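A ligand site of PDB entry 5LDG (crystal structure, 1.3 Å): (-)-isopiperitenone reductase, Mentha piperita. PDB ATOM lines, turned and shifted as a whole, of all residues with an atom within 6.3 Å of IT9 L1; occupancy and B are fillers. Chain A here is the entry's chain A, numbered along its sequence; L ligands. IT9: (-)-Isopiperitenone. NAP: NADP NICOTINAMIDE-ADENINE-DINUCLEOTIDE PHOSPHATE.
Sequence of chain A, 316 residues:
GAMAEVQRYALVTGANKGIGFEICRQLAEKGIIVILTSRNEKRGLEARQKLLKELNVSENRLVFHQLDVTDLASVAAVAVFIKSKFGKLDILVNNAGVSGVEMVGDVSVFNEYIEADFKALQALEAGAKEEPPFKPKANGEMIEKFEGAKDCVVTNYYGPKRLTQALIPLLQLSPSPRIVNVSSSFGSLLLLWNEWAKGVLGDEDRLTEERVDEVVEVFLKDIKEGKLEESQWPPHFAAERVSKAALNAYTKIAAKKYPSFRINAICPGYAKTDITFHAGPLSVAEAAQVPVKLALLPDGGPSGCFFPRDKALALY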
ATOM      1  N   VAL A  98     -24.389  -8.133  -9.227  1.00  0.00           N
ATOM      2  CA  VAL A  98     -24.451  -7.142 -10.294  1.00  0.00           C
ATOM      3  C   VAL A  98     -23.344  -7.456 -11.307  1.00  0.00           C
ATOM      4  O   VAL A  98     -22.403  -8.169 -11.012  1.00  0.00           O
ATOM      5  CB  VAL A  98     -24.311  -5.688  -9.768  1.00  0.00           C
ATOM      6  CG1 VAL A  98     -25.463  -5.346  -8.822  1.00  0.00           C
ATOM      7  CG2 VAL A  98     -22.989  -5.482  -9.106  1.00  0.00           C
ATOM      8  N   SER A  99     -23.448  -6.871 -12.487  1.00  0.00           N
ATOM      9  CA  SER A  99     -22.567  -7.207 -13.601  1.00  0.00           C
ATOM     10  C   SER A  99     -21.313  -6.370 -13.691  1.00  0.00           C
ATOM     11  O   SER A  99     -20.353  -6.799 -14.349  1.00  0.00           O
ATOM     12  CB  SER A  99     -23.311  -7.043 -14.949  1.00  0.00           C
ATOM     13  OG  SER A  99     -23.540  -5.669 -15.231  1.00  0.00           O
ATOM     14  N   GLY A 100     -21.337  -5.158 -13.164  1.00  0.00           N
ATOM     15  CA  GLY A 100     -20.236  -4.225 -13.291  1.00  0.00           C
ATOM     16  C   GLY A 100     -20.186  -3.479 -14.610  1.00  0.00           C
ATOM     17  O   GLY A 100     -19.276  -2.668 -14.792  1.00  0.00           O
ATOM     18  N   PHE A 110     -24.774  -7.119 -24.853  1.00  0.00           N
ATOM     19  CA  PHE A 110     -24.478  -7.867 -23.627  1.00  0.00           C
ATOM     20  C   PHE A 110     -24.574  -9.377 -23.881  1.00  0.00           C
ATOM     21  O   PHE A 110     -23.680 -10.147 -23.500  1.00  0.00           O
ATOM     22  CB  PHE A 110     -25.440  -7.395 -22.541  1.00  0.00           C
ATOM     23  CG  PHE A 110     -25.147  -7.919 -21.158  1.00  0.00           C
ATOM     24  CD1 PHE A 110     -25.656  -9.126 -20.733  1.00  0.00           C
ATOM     25  CD2 PHE A 110     -24.387  -7.190 -20.254  1.00  0.00           C
ATOM     26  CE1 PHE A 110     -25.402  -9.591 -19.477  1.00  0.00           C
ATOM     27  CE2 PHE A 110     -24.176  -7.654 -18.986  1.00  0.00           C
ATOM     28  CZ  PHE A 110     -24.663  -8.848 -18.617  1.00  0.00           C
ATOM     29  N   ILE A 114     -21.908 -12.646 -23.746  1.00  0.00           N
ATOM     30  CA  ILE A 114     -22.159 -13.878 -22.995  1.00  0.00           C
ATOM     31  C   ILE A 114     -21.973 -15.086 -23.901  1.00  0.00           C
ATOM     32  O   ILE A 114     -21.327 -16.074 -23.524  1.00  0.00           O
ATOM     33  CB  ILE A 114     -23.581 -13.857 -22.392  1.00  0.00           C
ATOM     34  CG1 ILE A 114     -23.696 -12.714 -21.391  1.00  0.00           C
ATOM     35  CG2 ILE A 114     -23.914 -15.211 -21.757  1.00  0.00           C
ATOM     36  CD1 ILE A 114     -22.933 -12.952 -20.146  1.00  0.00           C
ATOM     37  N   PHE A 118     -19.255 -18.155 -23.418  1.00  0.00           N
ATOM     38  CA  PHE A 118     -19.563 -19.575 -23.274  1.00  0.00           C
ATOM     39  C   PHE A 118     -18.791 -20.402 -24.299  1.00  0.00           C
ATOM     40  O   PHE A 118     -18.251 -21.468 -23.972  1.00  0.00           O
ATOM     41  CB  PHE A 118     -21.084 -19.817 -23.385  1.00  0.00           C
ATOM     42  CG  PHE A 118     -21.852 -19.605 -22.071  1.00  0.00           C
ATOM     43  CD1 PHE A 118     -21.547 -20.310 -20.913  1.00  0.00           C
ATOM     44  CD2 PHE A 118     -22.919 -18.710 -22.027  1.00  0.00           C
ATOM     45  CE1 PHE A 118     -22.285 -20.121 -19.748  1.00  0.00           C
ATOM     46  CE2 PHE A 118     -23.659 -18.519 -20.871  1.00  0.00           C
ATOM     47  CZ  PHE A 118     -23.336 -19.199 -19.735  1.00  0.00           C
ATOM     48  N   SER A 183     -22.770 -18.242  -8.079  1.00  0.00           N
ATOM     49  CA  SER A 183     -21.582 -17.815  -8.771  1.00  0.00           C
ATOM     50  C   SER A 183     -21.850 -17.880 -10.276  1.00  0.00           C
ATOM     51  O   SER A 183     -22.990 -17.658 -10.699  1.00  0.00           O
ATOM     52  CB  SER A 183     -20.393 -18.634  -8.289  1.00  0.00           C
ATOM     53  OG  SER A 183     -19.227 -18.098  -8.840  1.00  0.00           O
ATOM     54  N   SER A 184     -20.829 -18.133 -11.055  1.00  0.00           N
ATOM     55  CA  SER A 184     -20.953 -18.176 -12.490  1.00  0.00           C
ATOM     56  C   SER A 184     -19.843 -19.055 -13.026  1.00  0.00           C
ATOM     57  O   SER A 184     -18.729 -18.992 -12.534  1.00  0.00           O
ATOM     58  CB  SER A 184     -20.772 -16.763 -13.105  1.00  0.00           C
ATOM     59  OG  SER A 184     -20.709 -16.864 -14.494  1.00  0.00           O
ATOM     60  N   SER A 185     -20.126 -19.728 -14.142  1.00  0.00           N
ATOM     61  CA  SER A 185     -19.083 -20.427 -14.901  1.00  0.00           C
ATOM     62  C   SER A 185     -17.996 -19.475 -15.357  1.00  0.00           C
ATOM     63  O   SER A 185     -16.851 -19.917 -15.583  1.00  0.00           O
ATOM     64  CB  SER A 185     -19.677 -21.144 -16.120  1.00  0.00           C
ATOM     65  OG  SER A 185     -20.514 -22.197 -15.676  1.00  0.00           O
ATOM     66  N   PHE A 186     -18.326 -18.189 -15.491  1.00  0.00           N
ATOM     67  CA  PHE A 186     -17.320 -17.228 -15.924  1.00  0.00           C
ATOM     68  C   PHE A 186     -16.327 -16.859 -14.831  1.00  0.00           C
ATOM     69  O   PHE A 186     -15.366 -16.163 -15.131  1.00  0.00           O
ATOM     70  CB  PHE A 186     -17.993 -16.003 -16.492  1.00  0.00           C
ATOM     71  CG  PHE A 186     -18.855 -16.291 -17.701  1.00  0.00           C
ATOM     72  CD1 PHE A 186     -18.534 -17.311 -18.577  1.00  0.00           C
ATOM     73  CD2 PHE A 186     -19.958 -15.514 -17.982  1.00  0.00           C
ATOM     74  CE1 PHE A 186     -19.308 -17.547 -19.715  1.00  0.00           C
ATOM     75  CE2 PHE A 186     -20.740 -15.746 -19.086  1.00  0.00           C
ATOM     76  CZ  PHE A 186     -20.410 -16.760 -19.974  1.00  0.00           C
ATOM     77  N   GLY A 187     -16.502 -17.375 -13.606  1.00  0.00           N
ATOM     78  CA  GLY A 187     -15.438 -17.336 -12.622  1.00  0.00           C
ATOM     79  C   GLY A 187     -14.356 -18.358 -12.830  1.00  0.00           C
ATOM     80  O   GLY A 187     -13.404 -18.400 -12.041  1.00  0.00           O
ATOM     81  N   PHE A 237     -15.998  -8.205 -19.277  1.00  0.00           N
ATOM     82  CA  PHE A 237     -16.577  -8.787 -18.051  1.00  0.00           C
ATOM     83  C   PHE A 237     -15.505  -8.971 -16.983  1.00  0.00           C
ATOM     84  O   PHE A 237     -15.493  -9.936 -16.224  1.00  0.00           O
ATOM     85  CB  PHE A 237     -17.303 -10.114 -18.315  1.00  0.00           C
ATOM     86  CG  PHE A 237     -18.671  -9.966 -18.932  1.00  0.00           C
ATOM     87  CD1 PHE A 237     -19.604  -9.092 -18.391  1.00  0.00           C
ATOM     88  CD2 PHE A 237     -19.035 -10.722 -20.020  1.00  0.00           C
ATOM     89  CE1 PHE A 237     -20.866  -8.960 -18.924  1.00  0.00           C
ATOM     90  CE2 PHE A 237     -20.336 -10.601 -20.576  1.00  0.00           C
ATOM     91  CZ  PHE A 237     -21.226  -9.706 -20.011  1.00  0.00           C
ATOM     92  N   GLU A 240     -16.803  -8.929 -13.269  1.00  0.00           N
ATOM     93  CA  GLU A 240     -17.631 -10.104 -13.049  1.00  0.00           C
ATOM     94  C   GLU A 240     -16.766 -11.351 -12.903  1.00  0.00           C
ATOM     95  O   GLU A 240     -16.969 -12.159 -11.985  1.00  0.00           O
ATOM     96  CB  GLU A 240     -18.635 -10.249 -14.204  1.00  0.00           C
ATOM     97  CG  GLU A 240     -19.434 -11.557 -14.203  1.00  0.00           C
ATOM     98  CD  GLU A 240     -20.458 -11.699 -13.115  1.00  0.00           C
ATOM     99  OE1 GLU A 240     -20.659 -10.729 -12.364  1.00  0.00           O
ATOM    100  OE2 GLU A 240     -21.100 -12.776 -13.052  1.00  0.00           O
ATOM    101  N   LYS A 244     -16.427 -13.351  -9.327  1.00  0.00           N
ATOM    102  CA  LYS A 244     -16.933 -14.719  -9.216  1.00  0.00           C
ATOM    103  C   LYS A 244     -15.809 -15.723  -8.970  1.00  0.00           C
ATOM    104  O   LYS A 244     -15.987 -16.688  -8.213  1.00  0.00           O
ATOM    105  CB  LYS A 244     -17.804 -15.071 -10.423  1.00  0.00           C
ATOM    106  CG  LYS A 244     -19.062 -14.237 -10.558  1.00  0.00           C
ATOM    107  CD  LYS A 244     -20.078 -14.395  -9.486  1.00  0.00           C
ATOM    108  CE  LYS A 244     -21.444 -13.834  -9.915  1.00  0.00           C
ATOM    109  NZ  LYS A 244     -22.520 -13.947  -8.850  1.00  0.00           N
ATOM    110  N   CYS A 267     -23.384 -22.476 -10.614  1.00  0.00           N
ATOM    111  CA  CYS A 267     -23.840 -21.656 -11.732  1.00  0.00           C
ATOM    112  C   CYS A 267     -25.254 -22.085 -12.062  1.00  0.00           C
ATOM    113  O   CYS A 267     -25.497 -23.276 -12.304  1.00  0.00           O
ATOM    114  CB  CYS A 267     -22.940 -21.828 -12.968  1.00  0.00           C
ATOM    115  SG  CYS A 267     -23.406 -20.789 -14.371  1.00  0.00           S
ATOM    116  N   GLY A 269     -26.970 -21.474 -14.751  1.00  0.00           N
ATOM    117  CA  GLY A 269     -27.230 -21.467 -16.172  1.00  0.00           C
ATOM    118  C   GLY A 269     -27.587 -20.075 -16.637  1.00  0.00           C
ATOM    119  O   GLY A 269     -27.795 -19.158 -15.862  1.00  0.00           O
ATOM    120  N   TYR A 270     -27.711 -19.941 -17.935  1.00  0.00           N
ATOM    121  CA  TYR A 270     -27.951 -18.650 -18.586  1.00  0.00           C
ATOM    122  C   TYR A 270     -29.475 -18.483 -18.644  1.00  0.00           C
ATOM    123  O   TYR A 270     -30.175 -19.229 -19.357  1.00  0.00           O
ATOM    124  CB  TYR A 270     -27.300 -18.706 -19.956  1.00  0.00           C
ATOM    125  CG  TYR A 270     -27.399 -17.486 -20.804  1.00  0.00           C
ATOM    126  CD1 TYR A 270     -27.709 -16.232 -20.277  1.00  0.00           C
ATOM    127  CD2 TYR A 270     -27.147 -17.576 -22.179  1.00  0.00           C
ATOM    128  CE1 TYR A 270     -27.790 -15.103 -21.105  1.00  0.00           C
ATOM    129  CE2 TYR A 270     -27.219 -16.463 -22.990  1.00  0.00           C
ATOM    130  CZ  TYR A 270     -27.514 -15.241 -22.442  1.00  0.00           C
ATOM    131  OH  TYR A 270     -27.585 -14.127 -23.285  1.00  0.00           O
ATOM    132  N   ALA A 271     -29.995 -17.523 -17.872  1.00  0.00           N
ATOM    133  CA  ALA A 271     -31.427 -17.438 -17.622  1.00  0.00           C
ATOM    134  C   ALA A 271     -31.937 -16.028 -17.844  1.00  0.00           C
ATOM    135  O   ALA A 271     -31.218 -15.048 -17.651  1.00  0.00           O
ATOM    136  CB  ALA A 271     -31.697 -17.830 -16.182  1.00  0.00           C
ATOM    137  N   ILE A 275     -30.622  -8.950 -15.400  1.00  0.00           N
ATOM    138  CA  ILE A 275     -29.174  -8.839 -15.629  1.00  0.00           C
ATOM    139  C   ILE A 275     -28.812  -9.226 -17.054  1.00  0.00           C
ATOM    140  O   ILE A 275     -27.803  -8.753 -17.585  1.00  0.00           O
ATOM    141  CB  ILE A 275     -28.387  -9.643 -14.575  1.00  0.00           C
ATOM    142  CG1 ILE A 275     -27.017  -9.027 -14.347  1.00  0.00           C
ATOM    143  CG2 ILE A 275     -28.276 -11.113 -14.940  1.00  0.00           C
ATOM    144  CD1 ILE A 275     -26.295  -9.640 -13.157  1.00  0.00           C
ATOM    145  N   THR A 276     -29.599 -10.098 -17.693  1.00  0.00           N
ATOM    146  CA  THR A 276     -29.345 -10.530 -19.056  1.00  0.00           C
ATOM    147  C   THR A 276     -30.300  -9.876 -20.061  1.00  0.00           C
ATOM    148  O   THR A 276     -30.375 -10.331 -21.214  1.00  0.00           O
ATOM    149  CB  THR A 276     -29.492 -12.039 -19.191  1.00  0.00           C
ATOM    150  OG1 THR A 276     -30.851 -12.369 -18.951  1.00  0.00           O
ATOM    151  CG2 THR A 276     -28.552 -12.816 -18.310  1.00  0.00           C
HETATM  152  C4  IT9 L   1     -23.341 -12.870 -15.076  1.00  0.00           C
HETATM  153  C5  IT9 L   1     -24.865 -13.005 -15.283  1.00  0.00           C
HETATM  154  C6  IT9 L   1     -25.144 -13.638 -16.644  1.00  0.00           C
HETATM  155  C7  IT9 L   1     -22.813 -11.761 -15.964  1.00  0.00           C
HETATM  156  C8  IT9 L   1     -22.947 -10.472 -15.594  1.00  0.00           C
HETATM  157  C9  IT9 L   1     -22.093 -12.131 -17.209  1.00  0.00           C
HETATM  158  C   IT9 L   1     -24.871 -15.811 -17.966  1.00  0.00           C
HETATM  159  O   IT9 L   1     -21.480 -14.383 -14.939  1.00  0.00           O
HETATM  160  C1  IT9 L   1     -24.378 -14.898 -16.884  1.00  0.00           C
HETATM  161  C2  IT9 L   1     -23.248 -15.145 -16.221  1.00  0.00           C
HETATM  162  C3  IT9 L   1     -22.628 -14.203 -15.325  1.00  0.00           C
HETATM  163  PA  NAP L   2     -31.345  -9.764 -11.404  1.00  0.00           P
HETATM  164  O1A NAP L   2     -30.670  -8.523 -11.814  1.00  0.00           O
HETATM  165  O2A NAP L   2     -32.617 -10.005 -11.843  1.00  0.00           O
HETATM  166  O5B NAP L   2     -31.416  -9.838  -9.781  1.00  0.00           O
HETATM  167  C5B NAP L   2     -30.278  -9.377  -9.014  1.00  0.00           C
HETATM  168  C4B NAP L   2     -30.779  -9.233  -7.616  1.00  0.00           C
HETATM  169  O4B NAP L   2     -29.654  -8.835  -6.795  1.00  0.00           O
HETATM  170  C3B NAP L   2     -31.863  -8.162  -7.452  1.00  0.00           C
HETATM  171  O3B NAP L   2     -32.762  -8.586  -6.427  1.00  0.00           O
HETATM  172  C2B NAP L   2     -31.016  -6.986  -6.995  1.00  0.00           C
HETATM  173  O2B NAP L   2     -31.769  -6.012  -6.264  1.00  0.00           O
HETATM  174  C1B NAP L   2     -30.081  -7.718  -6.062  1.00  0.00           C
HETATM  175  N9A NAP L   2     -28.943  -6.927  -5.615  1.00  0.00           N
HETATM  176  C8A NAP L   2     -27.996  -6.255  -6.346  1.00  0.00           C
HETATM  177  N7A NAP L   2     -27.145  -5.580  -5.602  1.00  0.00           N
HETATM  178  C5A NAP L   2     -27.581  -5.832  -4.302  1.00  0.00           C
HETATM  179  C6A NAP L   2     -27.115  -5.388  -3.034  1.00  0.00           C
HETATM  180  N6A NAP L   2     -26.129  -4.494  -2.865  1.00  0.00           N
HETATM  181  N1A NAP L   2     -27.739  -5.873  -1.946  1.00  0.00           N
HETATM  182  C2A NAP L   2     -28.787  -6.676  -2.094  1.00  0.00           C
HETATM  183  N3A NAP L   2     -29.344  -7.110  -3.231  1.00  0.00           N
HETATM  184  C4A NAP L   2     -28.670  -6.653  -4.305  1.00  0.00           C
HETATM  185  O3  NAP L   2     -30.399 -10.932 -11.874  1.00  0.00           O
HETATM  186  PN  NAP L   2     -30.279 -12.486 -11.564  1.00  0.00           P
HETATM  187  O1N NAP L   2     -31.469 -12.936 -10.844  1.00  0.00           O
HETATM  188  O2N NAP L   2     -29.935 -13.141 -12.843  1.00  0.00           O
HETATM  189  O5D NAP L   2     -29.034 -12.466 -10.579  1.00  0.00           O
HETATM  190  C5D NAP L   2     -28.984 -13.363  -9.419  1.00  0.00           C
HETATM  191  C4D NAP L   2     -27.630 -13.996  -9.346  1.00  0.00           C
HETATM  192  O4D NAP L   2     -27.470 -14.945 -10.440  1.00  0.00           O
HETATM  193  C3D NAP L   2     -26.450 -13.004  -9.473  1.00  0.00           C
HETATM  194  O3D NAP L   2     -25.441 -13.300  -8.482  1.00  0.00           O
HETATM  195  C2D NAP L   2     -25.877 -13.313 -10.857  1.00  0.00           C
HETATM  196  O2D NAP L   2     -24.484 -13.074 -10.965  1.00  0.00           O
HETATM  197  C1D NAP L   2     -26.177 -14.797 -10.958  1.00  0.00           C
HETATM  198  N1N NAP L   2     -26.149 -15.380 -12.329  1.00  0.00           N
HETATM  199  C2N NAP L   2     -27.139 -15.087 -13.200  1.00  0.00           C
HETATM  200  C3N NAP L   2     -27.127 -15.642 -14.457  1.00  0.00           C
HETATM  201  C7N NAP L   2     -28.209 -15.431 -15.465  1.00  0.00           C
HETATM  202  O7N NAP L   2     -28.051 -15.899 -16.609  1.00  0.00           O
HETATM  203  N7N NAP L   2     -29.279 -14.761 -15.134  1.00  0.00           N
HETATM  204  C4N NAP L   2     -26.073 -16.508 -14.808  1.00  0.00           C
HETATM  205  C5N NAP L   2     -25.069 -16.788 -13.887  1.00  0.00           C
HETATM  206  C6N NAP L   2     -25.131 -16.205 -12.643  1.00  0.00           C
HETATM  207  P2B NAP L   2     -32.366  -4.664  -6.967  1.00  0.00           P
HETATM  208  O1X NAP L   2     -33.645  -4.988  -7.503  1.00  0.00           O
HETATM  209  O2X NAP L   2     -31.383  -4.239  -7.993  1.00  0.00           O
HETATM  210  O3X NAP L   2     -32.404  -3.727  -5.813  1.00  0.00           O
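An oxygen (O) of IT9 L1 sits close to the side-chain carboxylate (OE2) of Glu 240 (2.5 Å).
OG of Ser 184 lies within hydrogen-bond range of O of IT9 L1 (2.6 Å).
O3D of NAP L2 lies within hydrogen-bond range of NZ of Lys 244 (3.0 Å).
O7N of NAP L2 lies within hydrogen-bond range of N of Ala 271, 2.8 Å away.
O of Ala 271 lies within hydrogen-bond range of N7N of NAP L2, at 3.2 Å.
Merely in contact with IT9 L1: Ser 99 (3.5 Å), Phe 110 (3.8 Å), Ile 114 (3.2 Å), Phe 186 (3.6 Å), Phe 237 (3.8 Å), Tyr 270 (3.7 Å), Ile 275 (3.9 Å) and Thr 276 (3.9 Å).
Within 4 Å of IT9 L1: Ser 99, Phe 110, Ile 114, Ser 184, Phe 186, Phe 237, Glu 240, Tyr 270, Ile 275 and Thr 276.
The nearest printed residue that does not touch IT9 L1 is Phe 118 (4.1 Å).
OG of Ser 184 lies within hydrogen-bond range of N of Phe 186.
OG1 of Thr 276 sits at hydrogen-bond distance from O of Ala 271, at 3.0 Å.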
